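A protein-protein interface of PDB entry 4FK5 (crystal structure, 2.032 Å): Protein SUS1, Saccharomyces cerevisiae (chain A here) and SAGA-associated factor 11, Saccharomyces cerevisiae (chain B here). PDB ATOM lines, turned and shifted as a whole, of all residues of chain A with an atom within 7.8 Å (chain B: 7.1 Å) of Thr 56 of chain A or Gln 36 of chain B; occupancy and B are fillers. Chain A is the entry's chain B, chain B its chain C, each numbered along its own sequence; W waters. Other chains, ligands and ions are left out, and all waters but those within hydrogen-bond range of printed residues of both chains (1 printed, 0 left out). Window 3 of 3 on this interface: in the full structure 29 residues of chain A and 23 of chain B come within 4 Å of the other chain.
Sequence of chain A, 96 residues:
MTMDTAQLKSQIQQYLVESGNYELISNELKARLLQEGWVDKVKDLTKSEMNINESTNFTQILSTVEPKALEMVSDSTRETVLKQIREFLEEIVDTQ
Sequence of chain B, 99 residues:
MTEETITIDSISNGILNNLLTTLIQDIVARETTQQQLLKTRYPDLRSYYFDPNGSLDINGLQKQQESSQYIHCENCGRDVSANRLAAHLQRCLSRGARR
Thr 56 of chain A touches three residues of chain B. Printed residues of chain A within 4 Å of Gln 36 of chain B: Thr 56. Of the printed residues of chain A, Gln 35 of chain B touches Met 50 (3.6 Å) and Thr 56 (3.6 Å). Of the printed residues of chain B, Met 50 of chain A touches Glu 31, Thr 32 and Gln 35. The nearest residue of chain B that does not touch Thr 56 of chain A is Lys 39 of chain B (4.2 Å). The nearest residue of chain A that does not touch Gln 36 of chain B is Met 50 of chain A (5.9 Å). The nearest printed residue of chain A that does not touch Thr 32 of chain B is Ile 61 of chain A (4.1 Å).
Of the 13 printed residues of chain A, 3 touch a printed residue of chain B. Hydrophobic or aromatic side chains of chain A that line the printed part of chain B: Met 50 and Phe 58. Hydrophobic or aromatic side chains of chain B that line the printed part of chain A: Val 28. Among the printed residues, no Asp or Glu carboxylate lies within 4 Å of a Lys or Arg side-chain nitrogen of the other chain.
Water W1 bridges OG1 of Thr 32 of chain B (2.6 Å) and O of Thr 56 of chain A (3.5 Å).
Among the printed residues, pairs that only touch across the chains: Thr 56 of chain A with Thr 32 of chain B (3.4 Å), Met 50 of chain A with Gln 35 of chain B (3.6 Å), Phe 58 of chain A with Val 28 of chain B (3.6 Å), Thr 56 of chain A with Gln 35 of chain B (3.6 Å), Thr 56 of chain A with Gln 36 of chain B (3.8 Å), Met 50 of chain A with Glu 31 of chain B (3.8 Å), Phe 58 of chain A with Thr 32 of chain B (3.9 Å) and Met 50 of chain A with Thr 32 of chain B (3.9 Å).
O of Met 50 of chain A is in hydrogen-bond range of N of Ser 55 of chain A, 3.1 Å away. The backbone carbonyl oxygen of Val 28 of chain B lies within hydrogen-bond range of the side-chain hydroxyl of Thr 32 of chain B (3.2 Å). The backbone carbonyl oxygen (O) of Gln 36 of chain B lies within hydrogen-bond range of the side-chain hydroxyl (OG1) of Thr 40 of chain B (2.7 Å).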
ATOM      1  N   GLU A  49      16.512  33.560 -17.919  1.00  0.00           N
ATOM      2  CA  GLU A  49      16.096  33.632 -16.546  1.00  0.00           C
ATOM      3  C   GLU A  49      15.851  32.266 -15.919  1.00  0.00           C
ATOM      4  O   GLU A  49      16.127  32.080 -14.714  1.00  0.00           O
ATOM      5  CB  GLU A  49      14.882  34.540 -16.365  1.00  0.00           C
ATOM      6  CG  GLU A  49      15.174  36.015 -16.652  1.00  0.00           C
ATOM      7  CD  GLU A  49      16.046  36.686 -15.611  1.00  0.00           C
ATOM      8  OE1 GLU A  49      16.525  36.020 -14.662  1.00  0.00           O
ATOM      9  OE2 GLU A  49      16.241  37.887 -15.740  1.00  0.00           O
ATOM     10  N   MET A  50      15.382  31.299 -16.702  1.00  0.00           N
ATOM     11  CA  MET A  50      15.291  29.907 -16.205  1.00  0.00           C
ATOM     12  C   MET A  50      16.698  29.330 -15.786  1.00  0.00           C
ATOM     13  O   MET A  50      16.826  28.620 -14.756  1.00  0.00           O
ATOM     14  CB  MET A  50      14.646  28.994 -17.244  1.00  0.00           C
ATOM     15  CG  MET A  50      13.180  29.324 -17.486  1.00  0.00           C
ATOM     16  SD  MET A  50      12.268  28.088 -18.395  1.00  0.00           S
ATOM     17  CE  MET A  50      12.939  28.309 -20.073  1.00  0.00           C
ATOM     18  N   ASN A  51      17.695  29.562 -16.633  1.00  0.00           N
ATOM     19  CA  ASN A  51      19.066  29.162 -16.358  1.00  0.00           C
ATOM     20  C   ASN A  51      19.590  29.844 -15.090  1.00  0.00           C
ATOM     21  O   ASN A  51      20.076  29.209 -14.188  1.00  0.00           O
ATOM     22  CB  ASN A  51      19.972  29.547 -17.528  1.00  0.00           C
ATOM     23  CG  ASN A  51      21.422  29.220 -17.267  1.00  0.00           C
ATOM     24  OD1 ASN A  51      21.804  28.055 -17.271  1.00  0.00           O
ATOM     25  ND2 ASN A  51      22.244  30.251 -17.033  1.00  0.00           N
ATOM     26  N   ASN A  53      18.021  31.191 -12.487  1.00  0.00           N
ATOM     27  CA  ASN A  53      17.358  30.867 -11.202  1.00  0.00           C
ATOM     28  C   ASN A  53      17.207  29.372 -11.025  1.00  0.00           C
ATOM     29  O   ASN A  53      16.557  28.900 -10.047  1.00  0.00           O
ATOM     30  CB  ASN A  53      15.959  31.532 -11.123  1.00  0.00           C
ATOM     31  CG  ASN A  53      16.024  33.055 -11.085  1.00  0.00           C
ATOM     32  OD1 ASN A  53      16.330  33.653 -10.048  1.00  0.00           O
ATOM     33  ND2 ASN A  53      15.743  33.701 -12.243  1.00  0.00           N
ATOM     34  N   GLU A  54      17.722  28.622 -12.005  1.00  0.00           N
ATOM     35  CA  GLU A  54      17.596  27.148 -12.054  1.00  0.00           C
ATOM     36  C   GLU A  54      16.196  26.678 -11.718  1.00  0.00           C
ATOM     37  O   GLU A  54      15.986  25.830 -10.833  1.00  0.00           O
ATOM     38  CB  GLU A  54      18.624  26.500 -11.128  1.00  0.00           C
ATOM     39  CG  GLU A  54      19.971  27.158 -11.194  1.00  0.00           C
ATOM     40  CD  GLU A  54      20.879  26.673 -10.099  1.00  0.00           C
ATOM     41  OE1 GLU A  54      21.683  25.755 -10.379  1.00  0.00           O
ATOM     42  OE2 GLU A  54      20.729  27.148  -8.946  1.00  0.00           O
ATOM     43  N   SER A  55      15.226  27.178 -12.486  1.00  0.00           N
ATOM     44  CA  SER A  55      13.878  26.917 -12.214  1.00  0.00           C
ATOM     45  C   SER A  55      13.079  27.018 -13.514  1.00  0.00           C
ATOM     46  O   SER A  55      13.433  27.793 -14.421  1.00  0.00           O
ATOM     47  CB  SER A  55      13.362  27.911 -11.166  1.00  0.00           C
ATOM     48  OG  SER A  55      12.030  27.585 -10.777  1.00  0.00           O
ATOM     49  N   THR A  56      12.043  26.194 -13.612  1.00  0.00           N
ATOM     50  CA  THR A  56      11.002  26.349 -14.623  1.00  0.00           C
ATOM     51  C   THR A  56       9.647  26.776 -13.980  1.00  0.00           C
ATOM     52  O   THR A  56       8.604  26.812 -14.663  1.00  0.00           O
ATOM     53  CB  THR A  56      10.823  25.037 -15.410  1.00  0.00           C
ATOM     54  OG1 THR A  56      10.481  23.980 -14.517  1.00  0.00           O
ATOM     55  CG2 THR A  56      12.113  24.671 -16.182  1.00  0.00           C
ATOM     56  N   ASN A  57       9.651  27.088 -12.674  1.00  0.00           N
ATOM     57  CA  ASN A  57       8.400  27.465 -11.986  1.00  0.00           C
ATOM     58  C   ASN A  57       7.849  28.761 -12.554  1.00  0.00           C
ATOM     59  O   ASN A  57       8.510  29.829 -12.460  1.00  0.00           O
ATOM     60  CB  ASN A  57       8.596  27.637 -10.478  1.00  0.00           C
ATOM     61  CG  ASN A  57       7.306  27.995  -9.771  1.00  0.00           C
ATOM     62  OD1 ASN A  57       6.592  27.113  -9.314  1.00  0.00           O
ATOM     63  ND2 ASN A  57       6.974  29.300  -9.719  1.00  0.00           N
ATOM     64  N   PHE A  58       6.646  28.689 -13.138  1.00  0.00           N
ATOM     65  CA  PHE A  58       6.078  29.839 -13.876  1.00  0.00           C
ATOM     66  C   PHE A  58       5.993  31.104 -13.033  1.00  0.00           C
ATOM     67  O   PHE A  58       6.429  32.171 -13.464  1.00  0.00           O
ATOM     68  CB  PHE A  58       4.673  29.509 -14.470  1.00  0.00           C
ATOM     69  CG  PHE A  58       4.011  30.702 -15.132  1.00  0.00           C
ATOM     70  CD1 PHE A  58       4.386  31.096 -16.414  1.00  0.00           C
ATOM     71  CD2 PHE A  58       3.094  31.477 -14.429  1.00  0.00           C
ATOM     72  CE1 PHE A  58       3.845  32.231 -16.987  1.00  0.00           C
ATOM     73  CE2 PHE A  58       2.517  32.588 -15.001  1.00  0.00           C
ATOM     74  CZ  PHE A  58       2.887  32.973 -16.280  1.00  0.00           C
ATOM     75  N   THR A  59       5.482  30.995 -11.813  1.00  0.00           N
ATOM     76  CA  THR A  59       5.275  32.168 -10.964  1.00  0.00           C
ATOM     77  C   THR A  59       6.579  32.873 -10.666  1.00  0.00           C
ATOM     78  O   THR A  59       6.674  34.104 -10.720  1.00  0.00           O
ATOM     79  CB  THR A  59       4.584  31.760  -9.650  1.00  0.00           C
ATOM     80  OG1 THR A  59       3.357  31.112  -9.969  1.00  0.00           O
ATOM     81  CG2 THR A  59       4.296  33.003  -8.708  1.00  0.00           C
ATOM     82  N   GLN A  60       7.594  32.095 -10.364  1.00  0.00           N
ATOM     83  CA  GLN A  60       8.920  32.647 -10.075  1.00  0.00           C
ATOM     84  C   GLN A  60       9.539  33.280 -11.331  1.00  0.00           C
ATOM     85  O   GLN A  60      10.045  34.412 -11.288  1.00  0.00           O
ATOM     86  CB  GLN A  60       9.853  31.524  -9.523  1.00  0.00           C
ATOM     87  CG  GLN A  60      11.120  32.044  -8.882  1.00  0.00           C
ATOM     88  CD  GLN A  60      12.154  30.934  -8.593  1.00  0.00           C
ATOM     89  OE1 GLN A  60      13.356  31.212  -8.531  1.00  0.00           O
ATOM     90  NE2 GLN A  60      11.679  29.662  -8.435  1.00  0.00           N
ATOM     91  N   ILE A  61       9.488  32.559 -12.455  1.00  0.00           N
ATOM     92  CA  ILE A  61      10.098  33.065 -13.689  1.00  0.00           C
ATOM     93  C   ILE A  61       9.372  34.333 -14.166  1.00  0.00           C
ATOM     94  O   ILE A  61       9.997  35.304 -14.488  1.00  0.00           O
ATOM     95  CB  ILE A  61      10.147  32.007 -14.792  1.00  0.00           C
ATOM     96  CG1 ILE A  61      10.939  30.797 -14.344  1.00  0.00           C
ATOM     97  CG2 ILE A  61      10.786  32.567 -16.055  1.00  0.00           C
ATOM     98  CD1 ILE A  61      12.362  31.145 -13.933  1.00  0.00           C
ATOM     99  N   LEU A  62       8.041  34.336 -14.146  1.00  0.00           N
ATOM    100  CA  LEU A  62       7.293  35.527 -14.599  1.00  0.00           C
ATOM    101  C   LEU A  62       7.677  36.781 -13.817  1.00  0.00           C
ATOM    102  O   LEU A  62       7.868  37.849 -14.397  1.00  0.00           O
ATOM    103  CB  LEU A  62       5.763  35.271 -14.507  1.00  0.00           C
ATOM    104  CG  LEU A  62       4.937  36.464 -14.981  1.00  0.00           C
ATOM    105  CD1 LEU A  62       5.005  36.565 -16.548  1.00  0.00           C
ATOM    106  CD2 LEU A  62       3.508  36.374 -14.467  1.00  0.00           C
ATOM    107  N   VAL B  28       5.863  33.419 -21.742  1.00  0.00           N
ATOM    108  CA  VAL B  28       6.570  32.817 -20.621  1.00  0.00           C
ATOM    109  C   VAL B  28       6.032  31.411 -20.262  1.00  0.00           C
ATOM    110  O   VAL B  28       6.818  30.484 -20.004  1.00  0.00           O
ATOM    111  CB  VAL B  28       6.521  33.698 -19.381  1.00  0.00           C
ATOM    112  CG1 VAL B  28       7.166  32.959 -18.185  1.00  0.00           C
ATOM    113  CG2 VAL B  28       7.256  35.016 -19.652  1.00  0.00           C
ATOM    114  N   GLU B  31       7.301  28.948 -22.782  1.00  0.00           N
ATOM    115  CA  GLU B  31       8.721  28.664 -22.537  1.00  0.00           C
ATOM    116  C   GLU B  31       8.943  27.739 -21.350  1.00  0.00           C
ATOM    117  O   GLU B  31       9.710  26.805 -21.445  1.00  0.00           O
ATOM    118  CB  GLU B  31       9.470  29.939 -22.235  1.00  0.00           C
ATOM    119  CG  GLU B  31       9.612  30.807 -23.413  1.00  0.00           C
ATOM    120  CD  GLU B  31      10.346  30.135 -24.499  1.00  0.00           C
ATOM    121  OE1 GLU B  31      11.360  29.486 -24.187  1.00  0.00           O
ATOM    122  OE2 GLU B  31       9.927  30.268 -25.668  1.00  0.00           O
ATOM    123  N   THR B  32       8.291  28.045 -20.239  1.00  0.00           N
ATOM    124  CA  THR B  32       8.490  27.302 -19.019  1.00  0.00           C
ATOM    125  C   THR B  32       7.937  25.859 -19.153  1.00  0.00           C
ATOM    126  O   THR B  32       8.618  24.905 -18.758  1.00  0.00           O
ATOM    127  CB  THR B  32       7.964  28.019 -17.751  1.00  0.00           C
ATOM    128  OG1 THR B  32       6.544  28.217 -17.795  1.00  0.00           O
ATOM    129  CG2 THR B  32       8.671  29.374 -17.551  1.00  0.00           C
ATOM    130  N   THR B  33       6.749  25.679 -19.745  1.00  0.00           N
ATOM    131  CA  THR B  33       6.241  24.314 -19.947  1.00  0.00           C
ATOM    132  C   THR B  33       7.149  23.503 -20.843  1.00  0.00           C
ATOM    133  O   THR B  33       7.418  22.328 -20.558  1.00  0.00           O
ATOM    134  CB  THR B  33       4.801  24.269 -20.515  1.00  0.00           C
ATOM    135  OG1 THR B  33       4.734  25.091 -21.661  1.00  0.00           O
ATOM    136  CG2 THR B  33       3.775  24.755 -19.471  1.00  0.00           C
ATOM    137  N   GLN B  34       7.690  24.112 -21.909  1.00  0.00           N
ATOM    138  CA  GLN B  34       8.498  23.366 -22.824  1.00  0.00           C
ATOM    139  C   GLN B  34       9.766  22.886 -22.132  1.00  0.00           C
ATOM    140  O   GLN B  34      10.296  21.834 -22.449  1.00  0.00           O
ATOM    141  CB  GLN B  34       8.916  24.232 -24.020  1.00  0.00           C
ATOM    142  CG  GLN B  34       7.889  24.350 -25.102  1.00  0.00           C
ATOM    143  CD  GLN B  34       8.378  25.262 -26.255  1.00  0.00           C
ATOM    144  OE1 GLN B  34       7.710  26.231 -26.613  1.00  0.00           O
ATOM    145  NE2 GLN B  34       9.572  24.997 -26.752  1.00  0.00           N
ATOM    146  N   GLN B  35      10.327  23.745 -21.297  1.00  0.00           N
ATOM    147  CA  GLN B  35      11.637  23.464 -20.671  1.00  0.00           C
ATOM    148  C   GLN B  35      11.424  22.412 -19.574  1.00  0.00           C
ATOM    149  O   GLN B  35      12.274  21.524 -19.383  1.00  0.00           O
ATOM    150  CB  GLN B  35      12.249  24.778 -20.086  1.00  0.00           C
ATOM    151  CG  GLN B  35      13.638  24.662 -19.456  1.00  0.00           C
ATOM    152  CD  GLN B  35      14.694  24.178 -20.409  1.00  0.00           C
ATOM    153  OE1 GLN B  35      14.456  24.013 -21.592  1.00  0.00           O
ATOM    154  NE2 GLN B  35      15.868  23.911 -19.887  1.00  0.00           N
ATOM    155  N   GLN B  36      10.302  22.539 -18.847  1.00  0.00           N
ATOM    156  CA  GLN B  36       9.926  21.563 -17.846  1.00  0.00           C
ATOM    157  C   GLN B  36       9.813  20.174 -18.501  1.00  0.00           C
ATOM    158  O   GLN B  36      10.294  19.184 -17.949  1.00  0.00           O
ATOM    159  CB  GLN B  36       8.623  21.944 -17.137  1.00  0.00           C
ATOM    160  CG  GLN B  36       8.418  21.136 -15.889  1.00  0.00           C
ATOM    161  CD  GLN B  36       7.007  21.150 -15.374  1.00  0.00           C
ATOM    162  OE1 GLN B  36       6.078  21.005 -16.119  1.00  0.00           O
ATOM    163  NE2 GLN B  36       6.861  21.188 -14.020  1.00  0.00           N
ATOM    164  N   LEU B  37       9.203  20.116 -19.683  1.00  0.00           N
ATOM    165  CA  LEU B  37       9.116  18.872 -20.442  1.00  0.00           C
ATOM    166  C   LEU B  37      10.494  18.341 -20.816  1.00  0.00           C
ATOM    167  O   LEU B  37      10.802  17.181 -20.534  1.00  0.00           O
ATOM    168  CB  LEU B  37       8.235  19.026 -21.707  1.00  0.00           C
ATOM    169  CG  LEU B  37       8.055  17.755 -22.551  1.00  0.00           C
ATOM    170  CD1 LEU B  37       7.488  16.639 -21.694  1.00  0.00           C
ATOM    171  CD2 LEU B  37       7.198  17.988 -23.827  1.00  0.00           C
ATOM    172  N   LEU B  38      11.330  19.172 -21.437  1.00  0.00           N
ATOM    173  CA  LEU B  38      12.653  18.718 -21.885  1.00  0.00           C
ATOM    174  C   LEU B  38      13.455  18.199 -20.682  1.00  0.00           C
ATOM    175  O   LEU B  38      14.087  17.145 -20.752  1.00  0.00           O
ATOM    176  CB  LEU B  38      13.447  19.838 -22.584  1.00  0.00           C
ATOM    177  CG  LEU B  38      13.135  20.145 -24.041  1.00  0.00           C
ATOM    178  CD1 LEU B  38      14.106  21.208 -24.537  1.00  0.00           C
ATOM    179  CD2 LEU B  38      13.202  18.890 -24.931  1.00  0.00           C
ATOM    180  N   LYS B  39      13.411  18.922 -19.574  1.00  0.00           N
ATOM    181  CA  LYS B  39      14.248  18.538 -18.402  1.00  0.00           C
ATOM    182  C   LYS B  39      13.722  17.236 -17.713  1.00  0.00           C
ATOM    183  O   LYS B  39      14.499  16.473 -17.134  1.00  0.00           O
ATOM    184  CB  LYS B  39      14.336  19.674 -17.381  1.00  0.00           C
ATOM    185  CG  LYS B  39      15.364  20.754 -17.716  1.00  0.00           C
ATOM    186  CD  LYS B  39      15.238  21.924 -16.734  1.00  0.00           C
ATOM    187  CE  LYS B  39      16.537  22.749 -16.600  1.00  0.00           C
ATOM    188  NZ  LYS B  39      16.285  24.151 -16.076  1.00  0.00           N
ATOM    189  N   THR B  40      12.413  17.016 -17.771  1.00  0.00           N
ATOM    190  CA  THR B  40      11.813  15.797 -17.217  1.00  0.00           C
ATOM    191  C   THR B  40      12.083  14.611 -18.139  1.00  0.00           C
ATOM    192  O   THR B  40      12.466  13.551 -17.708  1.00  0.00           O
ATOM    193  CB  THR B  40      10.308  15.964 -17.033  1.00  0.00           C
ATOM    194  OG1 THR B  40      10.076  17.105 -16.184  1.00  0.00           O
ATOM    195  CG2 THR B  40       9.693  14.676 -16.405  1.00  0.00           C
ATOM    196  N   ARG B  41      11.981  14.852 -19.422  1.00  0.00           N
ATOM    197  CA  ARG B  41      12.188  13.834 -20.418  1.00  0.00           C
ATOM    198  C   ARG B  41      13.664  13.431 -20.491  1.00  0.00           C
ATOM    199  O   ARG B  41      13.989  12.254 -20.655  1.00  0.00           O
ATOM    200  CB  ARG B  41      11.694  14.383 -21.748  1.00  0.00           C
ATOM    201  CG  ARG B  41      11.514  13.401 -22.833  1.00  0.00           C
ATOM    202  CD  ARG B  41      10.849  14.066 -24.023  1.00  0.00           C
ATOM    203  NE  ARG B  41       9.395  13.950 -24.034  1.00  0.00           N
ATOM    204  CZ  ARG B  41       8.641  14.198 -25.085  1.00  0.00           C
ATOM    205  NH1 ARG B  41       9.167  14.706 -26.212  1.00  0.00           N
ATOM    206  NH2 ARG B  41       7.349  14.008 -25.013  1.00  0.00           N
ATOM    207  N   TYR B  42      14.564  14.391 -20.364  1.00  0.00           N
ATOM    208  CA  TYR B  42      15.993  14.094 -20.470  1.00  0.00           C
ATOM    209  C   TYR B  42      16.760  14.693 -19.293  1.00  0.00           C
ATOM    210  O   TYR B  42      17.346  15.764 -19.421  1.00  0.00           O
ATOM    211  CB  TYR B  42      16.592  14.646 -21.773  1.00  0.00           C
ATOM    212  CG  TYR B  42      15.790  14.398 -23.003  1.00  0.00           C
ATOM    213  CD1 TYR B  42      15.738  13.143 -23.564  1.00  0.00           C
ATOM    214  CD2 TYR B  42      15.107  15.456 -23.657  1.00  0.00           C
ATOM    215  CE1 TYR B  42      15.009  12.892 -24.707  1.00  0.00           C
ATOM    216  CE2 TYR B  42      14.385  15.227 -24.850  1.00  0.00           C
ATOM    217  CZ  TYR B  42      14.350  13.950 -25.380  1.00  0.00           C
ATOM    218  OH  TYR B  42      13.630  13.680 -26.525  1.00  0.00           O
HETATM  219  O   HOH W   1       5.484  26.504 -16.117  1.00  0.00           O
